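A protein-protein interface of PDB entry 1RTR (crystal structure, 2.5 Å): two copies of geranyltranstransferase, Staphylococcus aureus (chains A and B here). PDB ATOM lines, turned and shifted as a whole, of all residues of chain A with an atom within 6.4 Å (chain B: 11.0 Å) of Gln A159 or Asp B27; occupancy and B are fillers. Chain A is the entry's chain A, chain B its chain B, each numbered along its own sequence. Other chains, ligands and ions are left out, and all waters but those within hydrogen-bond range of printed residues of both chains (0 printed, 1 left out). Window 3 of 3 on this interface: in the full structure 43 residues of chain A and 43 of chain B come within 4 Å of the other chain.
The side-chain sulfur (SD) of Met A155 lies within hydrogen-bond range of the side-chain hydroxyl (OG1) of Thr B107.
The side-chain amide oxygen of Gln A159 lies close to the backbone carbonyl oxygen of Asp B27, at 3.3 Å.
No position is printed for both chains.
Of the 12 pairs that touch across the chains among the printed residues, none has its exchanged pair printed and touching as well.
Among the printed residues, pairs that only touch across the chains: Gln A154 with Leu B110, Met A155 with Thr B28, Met A155 with Gln B29, Met A155 with Leu B30, Met A155 with Trp B106, Met A155 with Leu B110, Leu A156 with Met B26, Met A158 with Trp B106, Gln A159 with Thr B28 and Gln A159 with Trp B106.
Gln A159 touches three residues of chain B.
Asp B27 touches just one residue of chain A: Gln A159.
Met A158 touches just one residue of chain B: Trp B106.
Ser A160 touches none of the printed residues of chain B.
Of the printed residues of chain A, Leu B110 touches Gln A154 (3.9 Å) and Met A155 (3.4 Å).
Printed residues of chain A within 4 Å of Thr B28: Met A155 (3.9 Å) and Gln A159 (3.5 Å).
Printed residues of chain A within 4 Å of Trp B106: Met A155, Met A158 and Gln A159.
Of the printed residues of chain A, Leu B30 touches Met A155 (3.2 Å).
Of the printed residues of chain A, Met B26 touches Leu A156.
Glu B31 touches none of the printed residues of chain A.
Ser B33 touches none of the printed residues of chain A.
The nearest residue of chain B that does not touch Gln A159 is Gln B29 (4.1 Å).
The backbone carbonyl oxygen (O) of Leu A156 sits at hydrogen-bond distance from the side-chain hydroxyl (OG) of Ser A160, at 2.9 Å.
The side-chain hydroxyl of Ser B24 lies close to the backbone NH of Met B26, at 3.2 Å.
The backbone carbonyl oxygen (O) of Tyr B103 lies close to the side-chain hydroxyl (OG1) of Thr B107 (3.5 Å).
Printed residues of chain B that touch a printed residue of chain A: Met B26, Asp B27, Thr B28, Gln B29, Leu B30, Trp B106, Thr B107 and Leu B110.
Hydrophobic or aromatic side chains of chain B within 4 Å of the printed part of chain A: Met B26, Leu B30, Trp B106 and Leu B110.
Of the 10 printed residues of chain A, 5 touch a printed residue of chain B.
Hydrophobic or aromatic side chains of chain A that line the printed part of chain B: Met A155, Leu A156 and Met A158.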
ATOM      1  N   GLN A 154     -14.899  23.926  -2.810  1.00  0.00           N
ATOM      2  CA  GLN A 154     -15.494  25.252  -2.943  1.00  0.00           C
ATOM      3  C   GLN A 154     -16.100  25.676  -1.618  1.00  0.00           C
ATOM      4  O   GLN A 154     -16.016  26.839  -1.261  1.00  0.00           O
ATOM      5  CB  GLN A 154     -16.572  25.291  -4.024  1.00  0.00           C
ATOM      6  CG  GLN A 154     -16.198  26.044  -5.302  1.00  0.00           C
ATOM      7  CD  GLN A 154     -15.778  27.496  -5.074  1.00  0.00           C
ATOM      8  OE1 GLN A 154     -16.533  28.306  -4.524  1.00  0.00           O
ATOM      9  NE2 GLN A 154     -14.581  27.827  -5.523  1.00  0.00           N
ATOM     10  N   MET A 155     -16.720  24.741  -0.896  1.00  0.00           N
ATOM     11  CA  MET A 155     -17.278  25.061   0.421  1.00  0.00           C
ATOM     12  C   MET A 155     -16.144  25.516   1.334  1.00  0.00           C
ATOM     13  O   MET A 155     -16.191  26.625   1.867  1.00  0.00           O
ATOM     14  CB  MET A 155     -18.024  23.878   1.038  1.00  0.00           C
ATOM     15  CG  MET A 155     -19.527  23.860   0.775  1.00  0.00           C
ATOM     16  SD  MET A 155     -20.517  25.175   1.517  1.00  0.00           S
ATOM     17  CE  MET A 155     -20.345  24.843   3.275  1.00  0.00           C
ATOM     18  N   LEU A 156     -15.118  24.667   1.458  1.00  0.00           N
ATOM     19  CA  LEU A 156     -13.926  24.974   2.232  1.00  0.00           C
ATOM     20  C   LEU A 156     -13.278  26.295   1.819  1.00  0.00           C
ATOM     21  O   LEU A 156     -12.905  27.072   2.677  1.00  0.00           O
ATOM     22  CB  LEU A 156     -12.913  23.822   2.201  1.00  0.00           C
ATOM     23  CG  LEU A 156     -11.838  23.859   3.306  1.00  0.00           C
ATOM     24  CD1 LEU A 156     -12.419  24.234   4.669  1.00  0.00           C
ATOM     25  CD2 LEU A 156     -11.049  22.558   3.405  1.00  0.00           C
ATOM     26  N   ASP A 157     -13.163  26.555   0.516  1.00  0.00           N
ATOM     27  CA  ASP A 157     -12.596  27.812   0.045  1.00  0.00           C
ATOM     28  C   ASP A 157     -13.389  29.013   0.560  1.00  0.00           C
ATOM     29  O   ASP A 157     -12.803  29.941   1.107  1.00  0.00           O
ATOM     30  CB  ASP A 157     -12.514  27.846  -1.488  1.00  0.00           C
ATOM     31  CG  ASP A 157     -11.387  28.746  -2.000  1.00  0.00           C
ATOM     32  OD1 ASP A 157     -11.258  28.898  -3.232  1.00  0.00           O
ATOM     33  OD2 ASP A 157     -10.572  29.335  -1.258  1.00  0.00           O
ATOM     34  N   MET A 158     -14.712  28.977   0.385  1.00  0.00           N
ATOM     35  CA  MET A 158     -15.616  30.072   0.749  1.00  0.00           C
ATOM     36  C   MET A 158     -15.647  30.304   2.260  1.00  0.00           C
ATOM     37  O   MET A 158     -15.700  31.438   2.713  1.00  0.00           O
ATOM     38  CB  MET A 158     -17.047  29.793   0.253  1.00  0.00           C
ATOM     39  CG  MET A 158     -17.243  29.811  -1.245  1.00  0.00           C
ATOM     40  SD  MET A 158     -17.392  31.465  -1.878  1.00  0.00           S
ATOM     41  CE  MET A 158     -16.180  31.425  -3.142  1.00  0.00           C
ATOM     42  N   GLN A 159     -15.638  29.220   3.028  1.00  0.00           N
ATOM     43  CA  GLN A 159     -15.533  29.276   4.483  1.00  0.00           C
ATOM     44  C   GLN A 159     -14.240  29.967   4.950  1.00  0.00           C
ATOM     45  O   GLN A 159     -14.242  30.700   5.941  1.00  0.00           O
ATOM     46  CB  GLN A 159     -15.583  27.864   5.057  1.00  0.00           C
ATOM     47  CG  GLN A 159     -15.720  27.815   6.561  1.00  0.00           C
ATOM     48  CD  GLN A 159     -15.948  26.415   7.064  1.00  0.00           C
ATOM     49  OE1 GLN A 159     -15.008  25.746   7.490  1.00  0.00           O
ATOM     50  NE2 GLN A 159     -17.194  25.957   7.009  1.00  0.00           N
ATOM     51  N   SER A 160     -13.154  29.725   4.215  1.00  0.00           N
ATOM     52  CA  SER A 160     -11.824  30.239   4.532  1.00  0.00           C
ATOM     53  C   SER A 160     -11.591  31.681   4.102  1.00  0.00           C
ATOM     54  O   SER A 160     -10.558  32.261   4.440  1.00  0.00           O
ATOM     55  CB  SER A 160     -10.757  29.360   3.878  1.00  0.00           C
ATOM     56  OG  SER A 160     -10.790  28.057   4.420  1.00  0.00           O
ATOM     57  N   GLU A 161     -12.534  32.254   3.352  1.00  0.00           N
ATOM     58  CA  GLU A 161     -12.352  33.575   2.739  1.00  0.00           C
ATOM     59  C   GLU A 161     -12.009  34.646   3.771  1.00  0.00           C
ATOM     60  O   GLU A 161     -12.727  34.820   4.757  1.00  0.00           O
ATOM     61  CB  GLU A 161     -13.594  33.981   1.947  1.00  0.00           C
ATOM     62  CG  GLU A 161     -13.421  35.250   1.130  1.00  0.00           C
ATOM     63  CD  GLU A 161     -14.236  35.218  -0.148  1.00  0.00           C
ATOM     64  OE1 GLU A 161     -13.666  34.865  -1.211  1.00  0.00           O
ATOM     65  OE2 GLU A 161     -15.451  35.531  -0.085  1.00  0.00           O
ATOM     66  N   GLY A 162     -10.894  35.339   3.533  1.00  0.00           N
ATOM     67  CA  GLY A 162     -10.402  36.391   4.415  1.00  0.00           C
ATOM     68  C   GLY A 162     -10.010  35.925   5.811  1.00  0.00           C
ATOM     69  O   GLY A 162     -10.033  36.718   6.754  1.00  0.00           O
ATOM     70  N   GLN A 163      -9.680  34.639   5.947  1.00  0.00           N
ATOM     71  CA  GLN A 163      -9.134  34.092   7.189  1.00  0.00           C
ATOM     72  C   GLN A 163      -7.707  33.639   6.923  1.00  0.00           C
ATOM     73  O   GLN A 163      -7.370  33.300   5.785  1.00  0.00           O
ATOM     74  CB  GLN A 163      -9.955  32.902   7.705  1.00  0.00           C
ATOM     75  CG  GLN A 163     -11.456  33.136   7.810  1.00  0.00           C
ATOM     76  CD  GLN A 163     -11.831  34.007   8.994  1.00  0.00           C
ATOM     77  OE1 GLN A 163     -12.315  33.502  10.012  1.00  0.00           O
ATOM     78  NE2 GLN A 163     -11.614  35.317   8.866  1.00  0.00           N
ATOM     79  N   ASN B  22     -22.838  11.079   4.964  1.00  0.00           N
ATOM     80  CA  ASN B  22     -21.996  11.024   6.170  1.00  0.00           C
ATOM     81  C   ASN B  22     -21.208  12.318   6.382  1.00  0.00           C
ATOM     82  O   ASN B  22     -20.887  13.009   5.408  1.00  0.00           O
ATOM     83  CB  ASN B  22     -20.997   9.859   6.086  1.00  0.00           C
ATOM     84  CG  ASN B  22     -21.654   8.495   6.242  1.00  0.00           C
ATOM     85  OD1 ASN B  22     -22.533   8.305   7.082  1.00  0.00           O
ATOM     86  ND2 ASN B  22     -21.222   7.533   5.427  1.00  0.00           N
ATOM     87  N   LYS B  23     -20.894  12.638   7.642  1.00  0.00           N
ATOM     88  CA  LYS B  23     -19.999  13.759   7.956  1.00  0.00           C
ATOM     89  C   LYS B  23     -18.654  13.547   7.268  1.00  0.00           C
ATOM     90  O   LYS B  23     -18.173  12.409   7.151  1.00  0.00           O
ATOM     91  CB  LYS B  23     -19.769  13.925   9.467  1.00  0.00           C
ATOM     92  CG  LYS B  23     -20.913  13.483  10.375  1.00  0.00           C
ATOM     93  CD  LYS B  23     -20.370  12.697  11.581  1.00  0.00           C
ATOM     94  CE  LYS B  23     -21.493  12.003  12.380  1.00  0.00           C
ATOM     95  NZ  LYS B  23     -22.483  12.997  12.912  1.00  0.00           N
ATOM     96  N   SER B  24     -18.051  14.645   6.824  1.00  0.00           N
ATOM     97  CA  SER B  24     -16.846  14.582   6.009  1.00  0.00           C
ATOM     98  C   SER B  24     -15.645  15.199   6.732  1.00  0.00           C
ATOM     99  O   SER B  24     -15.811  16.036   7.626  1.00  0.00           O
ATOM    100  CB  SER B  24     -17.096  15.242   4.639  1.00  0.00           C
ATOM    101  OG  SER B  24     -16.151  16.260   4.341  1.00  0.00           O
ATOM    102  N   VAL B  25     -14.444  14.780   6.333  1.00  0.00           N
ATOM    103  CA  VAL B  25     -13.199  15.264   6.928  1.00  0.00           C
ATOM    104  C   VAL B  25     -12.951  16.775   6.786  1.00  0.00           C
ATOM    105  O   VAL B  25     -12.107  17.326   7.487  1.00  0.00           O
ATOM    106  CB  VAL B  25     -11.962  14.454   6.405  1.00  0.00           C
ATOM    107  CG1 VAL B  25     -11.346  15.081   5.150  1.00  0.00           C
ATOM    108  CG2 VAL B  25     -10.908  14.306   7.499  1.00  0.00           C
ATOM    109  N   MET B  26     -13.681  17.444   5.899  1.00  0.00           N
ATOM    110  CA  MET B  26     -13.357  18.831   5.558  1.00  0.00           C
ATOM    111  C   MET B  26     -13.940  19.853   6.532  1.00  0.00           C
ATOM    112  O   MET B  26     -13.578  21.037   6.489  1.00  0.00           O
ATOM    113  CB  MET B  26     -13.749  19.150   4.112  1.00  0.00           C
ATOM    114  CG  MET B  26     -13.107  18.214   3.092  1.00  0.00           C
ATOM    115  SD  MET B  26     -13.633  18.550   1.425  1.00  0.00           S
ATOM    116  CE  MET B  26     -12.664  19.979   1.136  1.00  0.00           C
ATOM    117  N   ASP B  27     -14.834  19.390   7.406  1.00  0.00           N
ATOM    118  CA  ASP B  27     -15.361  20.199   8.505  1.00  0.00           C
ATOM    119  C   ASP B  27     -16.030  21.505   8.043  1.00  0.00           C
ATOM    120  O   ASP B  27     -15.579  22.618   8.357  1.00  0.00           O
ATOM    121  CB  ASP B  27     -14.265  20.468   9.540  1.00  0.00           C
ATOM    122  CG  ASP B  27     -14.824  20.664  10.936  1.00  0.00           C
ATOM    123  OD1 ASP B  27     -15.326  21.781  11.212  1.00  0.00           O
ATOM    124  OD2 ASP B  27     -14.811  19.762  11.817  1.00  0.00           O
ATOM    125  N   THR B  28     -17.103  21.356   7.278  1.00  0.00           N
ATOM    126  CA  THR B  28     -17.887  22.499   6.819  1.00  0.00           C
ATOM    127  C   THR B  28     -19.348  22.228   7.111  1.00  0.00           C
ATOM    128  O   THR B  28     -19.696  21.215   7.717  1.00  0.00           O
ATOM    129  CB  THR B  28     -17.703  22.748   5.296  1.00  0.00           C
ATOM    130  OG1 THR B  28     -17.933  21.528   4.585  1.00  0.00           O
ATOM    131  CG2 THR B  28     -16.263  23.091   4.955  1.00  0.00           C
ATOM    132  N   GLN B  29     -20.205  23.126   6.646  1.00  0.00           N
ATOM    133  CA  GLN B  29     -21.637  22.961   6.837  1.00  0.00           C
ATOM    134  C   GLN B  29     -22.348  22.284   5.660  1.00  0.00           C
ATOM    135  O   GLN B  29     -23.577  22.166   5.677  1.00  0.00           O
ATOM    136  CB  GLN B  29     -22.273  24.304   7.165  1.00  0.00           C
ATOM    137  CG  GLN B  29     -21.827  24.866   8.499  1.00  0.00           C
ATOM    138  CD  GLN B  29     -22.603  26.098   8.890  1.00  0.00           C
ATOM    139  OE1 GLN B  29     -23.130  26.167   9.998  1.00  0.00           O
ATOM    140  NE2 GLN B  29     -22.679  27.078   7.987  1.00  0.00           N
ATOM    141  N   LEU B  30     -21.578  21.823   4.666  1.00  0.00           N
ATOM    142  CA  LEU B  30     -22.140  21.231   3.449  1.00  0.00           C
ATOM    143  C   LEU B  30     -23.074  20.075   3.751  1.00  0.00           C
ATOM    144  O   LEU B  30     -24.213  20.061   3.306  1.00  0.00           O
ATOM    145  CB  LEU B  30     -21.045  20.746   2.490  1.00  0.00           C
ATOM    146  CG  LEU B  30     -21.144  21.058   0.984  1.00  0.00           C
ATOM    147  CD1 LEU B  30     -20.312  20.079   0.197  1.00  0.00           C
ATOM    148  CD2 LEU B  30     -22.539  21.127   0.397  1.00  0.00           C
ATOM    149  N   GLU B  31     -22.583  19.120   4.527  1.00  0.00           N
ATOM    150  CA  GLU B  31     -23.313  17.896   4.781  1.00  0.00           C
ATOM    151  C   GLU B  31     -24.527  18.208   5.643  1.00  0.00           C
ATOM    152  O   GLU B  31     -25.585  17.598   5.488  1.00  0.00           O
ATOM    153  CB  GLU B  31     -22.403  16.863   5.434  1.00  0.00           C
ATOM    154  CG  GLU B  31     -21.377  16.238   4.490  1.00  0.00           C
ATOM    155  CD  GLU B  31     -20.215  17.163   4.122  1.00  0.00           C
ATOM    156  OE1 GLU B  31     -19.841  18.040   4.941  1.00  0.00           O
ATOM    157  OE2 GLU B  31     -19.668  17.011   2.996  1.00  0.00           O
ATOM    158  N   GLU B  32     -24.378  19.187   6.529  1.00  0.00           N
ATOM    159  CA  GLU B  32     -25.474  19.633   7.381  1.00  0.00           C
ATOM    160  C   GLU B  32     -26.578  20.293   6.567  1.00  0.00           C
ATOM    161  O   GLU B  32     -27.756  20.002   6.757  1.00  0.00           O
ATOM    162  CB  GLU B  32     -24.956  20.610   8.426  1.00  0.00           C
ATOM    163  CG  GLU B  32     -25.305  20.229   9.850  1.00  0.00           C
ATOM    164  CD  GLU B  32     -25.091  21.394  10.793  1.00  0.00           C
ATOM    165  OE1 GLU B  32     -23.934  21.558  11.274  1.00  0.00           O
ATOM    166  OE2 GLU B  32     -26.070  22.154  11.021  1.00  0.00           O
ATOM    167  N   SER B  33     -26.189  21.184   5.668  1.00  0.00           N
ATOM    168  CA  SER B  33     -27.137  21.855   4.801  1.00  0.00           C
ATOM    169  C   SER B  33     -27.832  20.845   3.873  1.00  0.00           C
ATOM    170  O   SER B  33     -29.050  20.903   3.690  1.00  0.00           O
ATOM    171  CB  SER B  33     -26.434  22.947   4.003  1.00  0.00           C
ATOM    172  OG  SER B  33     -27.308  23.522   3.060  1.00  0.00           O
ATOM    173  N   TYR B 103     -28.429  28.839   6.159  1.00  0.00           N
ATOM    174  CA  TYR B 103     -26.997  28.636   5.918  1.00  0.00           C
ATOM    175  C   TYR B 103     -26.386  29.651   4.983  1.00  0.00           C
ATOM    176  O   TYR B 103     -25.178  29.613   4.743  1.00  0.00           O
ATOM    177  CB  TYR B 103     -26.729  27.235   5.359  1.00  0.00           C
ATOM    178  CG  TYR B 103     -27.148  26.125   6.271  1.00  0.00           C
ATOM    179  CD1 TYR B 103     -28.367  25.469   6.083  1.00  0.00           C
ATOM    180  CD2 TYR B 103     -26.335  25.726   7.334  1.00  0.00           C
ATOM    181  CE1 TYR B 103     -28.769  24.440   6.932  1.00  0.00           C
ATOM    182  CE2 TYR B 103     -26.724  24.694   8.184  1.00  0.00           C
ATOM    183  CZ  TYR B 103     -27.943  24.063   7.976  1.00  0.00           C
ATOM    184  OH  TYR B 103     -28.331  23.053   8.816  1.00  0.00           O
ATOM    185  N   TRP B 106     -24.674  30.992  -0.620  1.00  0.00           N
ATOM    186  CA  TRP B 106     -23.589  30.220  -1.255  1.00  0.00           C
ATOM    187  C   TRP B 106     -23.557  28.766  -0.805  1.00  0.00           C
ATOM    188  O   TRP B 106     -23.356  27.868  -1.628  1.00  0.00           O
ATOM    189  CB  TRP B 106     -22.195  30.884  -1.153  1.00  0.00           C
ATOM    190  CG  TRP B 106     -21.683  31.204   0.235  1.00  0.00           C
ATOM    191  CD1 TRP B 106     -21.790  32.400   0.891  1.00  0.00           C
ATOM    192  CD2 TRP B 106     -20.949  30.338   1.112  1.00  0.00           C
ATOM    193  NE1 TRP B 106     -21.194  32.326   2.127  1.00  0.00           N
ATOM    194  CE2 TRP B 106     -20.666  31.072   2.292  1.00  0.00           C
ATOM    195  CE3 TRP B 106     -20.513  29.008   1.033  1.00  0.00           C
ATOM    196  CZ2 TRP B 106     -19.975  30.524   3.375  1.00  0.00           C
ATOM    197  CZ3 TRP B 106     -19.824  28.467   2.109  1.00  0.00           C
ATOM    198  CH2 TRP B 106     -19.561  29.226   3.264  1.00  0.00           C
ATOM    199  N   THR B 107     -23.790  28.539   0.483  1.00  0.00           N
ATOM    200  CA  THR B 107     -23.879  27.187   1.010  1.00  0.00           C
ATOM    201  C   THR B 107     -25.042  26.431   0.377  1.00  0.00           C
ATOM    202  O   THR B 107     -24.885  25.279  -0.056  1.00  0.00           O
ATOM    203  CB  THR B 107     -24.013  27.217   2.543  1.00  0.00           C
ATOM    204  OG1 THR B 107     -22.782  27.692   3.104  1.00  0.00           O
ATOM    205  CG2 THR B 107     -24.144  25.807   3.116  1.00  0.00           C
ATOM    206  N   LEU B 110     -24.338  25.295  -3.071  1.00  0.00           N
ATOM    207  CA  LEU B 110     -23.422  24.158  -3.067  1.00  0.00           C
ATOM    208  C   LEU B 110     -24.095  22.875  -2.555  1.00  0.00           C
ATOM    209  O   LEU B 110     -23.809  21.773  -3.053  1.00  0.00           O
ATOM    210  CB  LEU B 110     -22.123  24.477  -2.302  1.00  0.00           C
ATOM    211  CG  LEU B 110     -21.234  25.636  -2.805  1.00  0.00           C
ATOM    212  CD1 LEU B 110     -19.953  25.709  -2.007  1.00  0.00           C
ATOM    213  CD2 LEU B 110     -20.904  25.597  -4.300  1.00  0.00           C
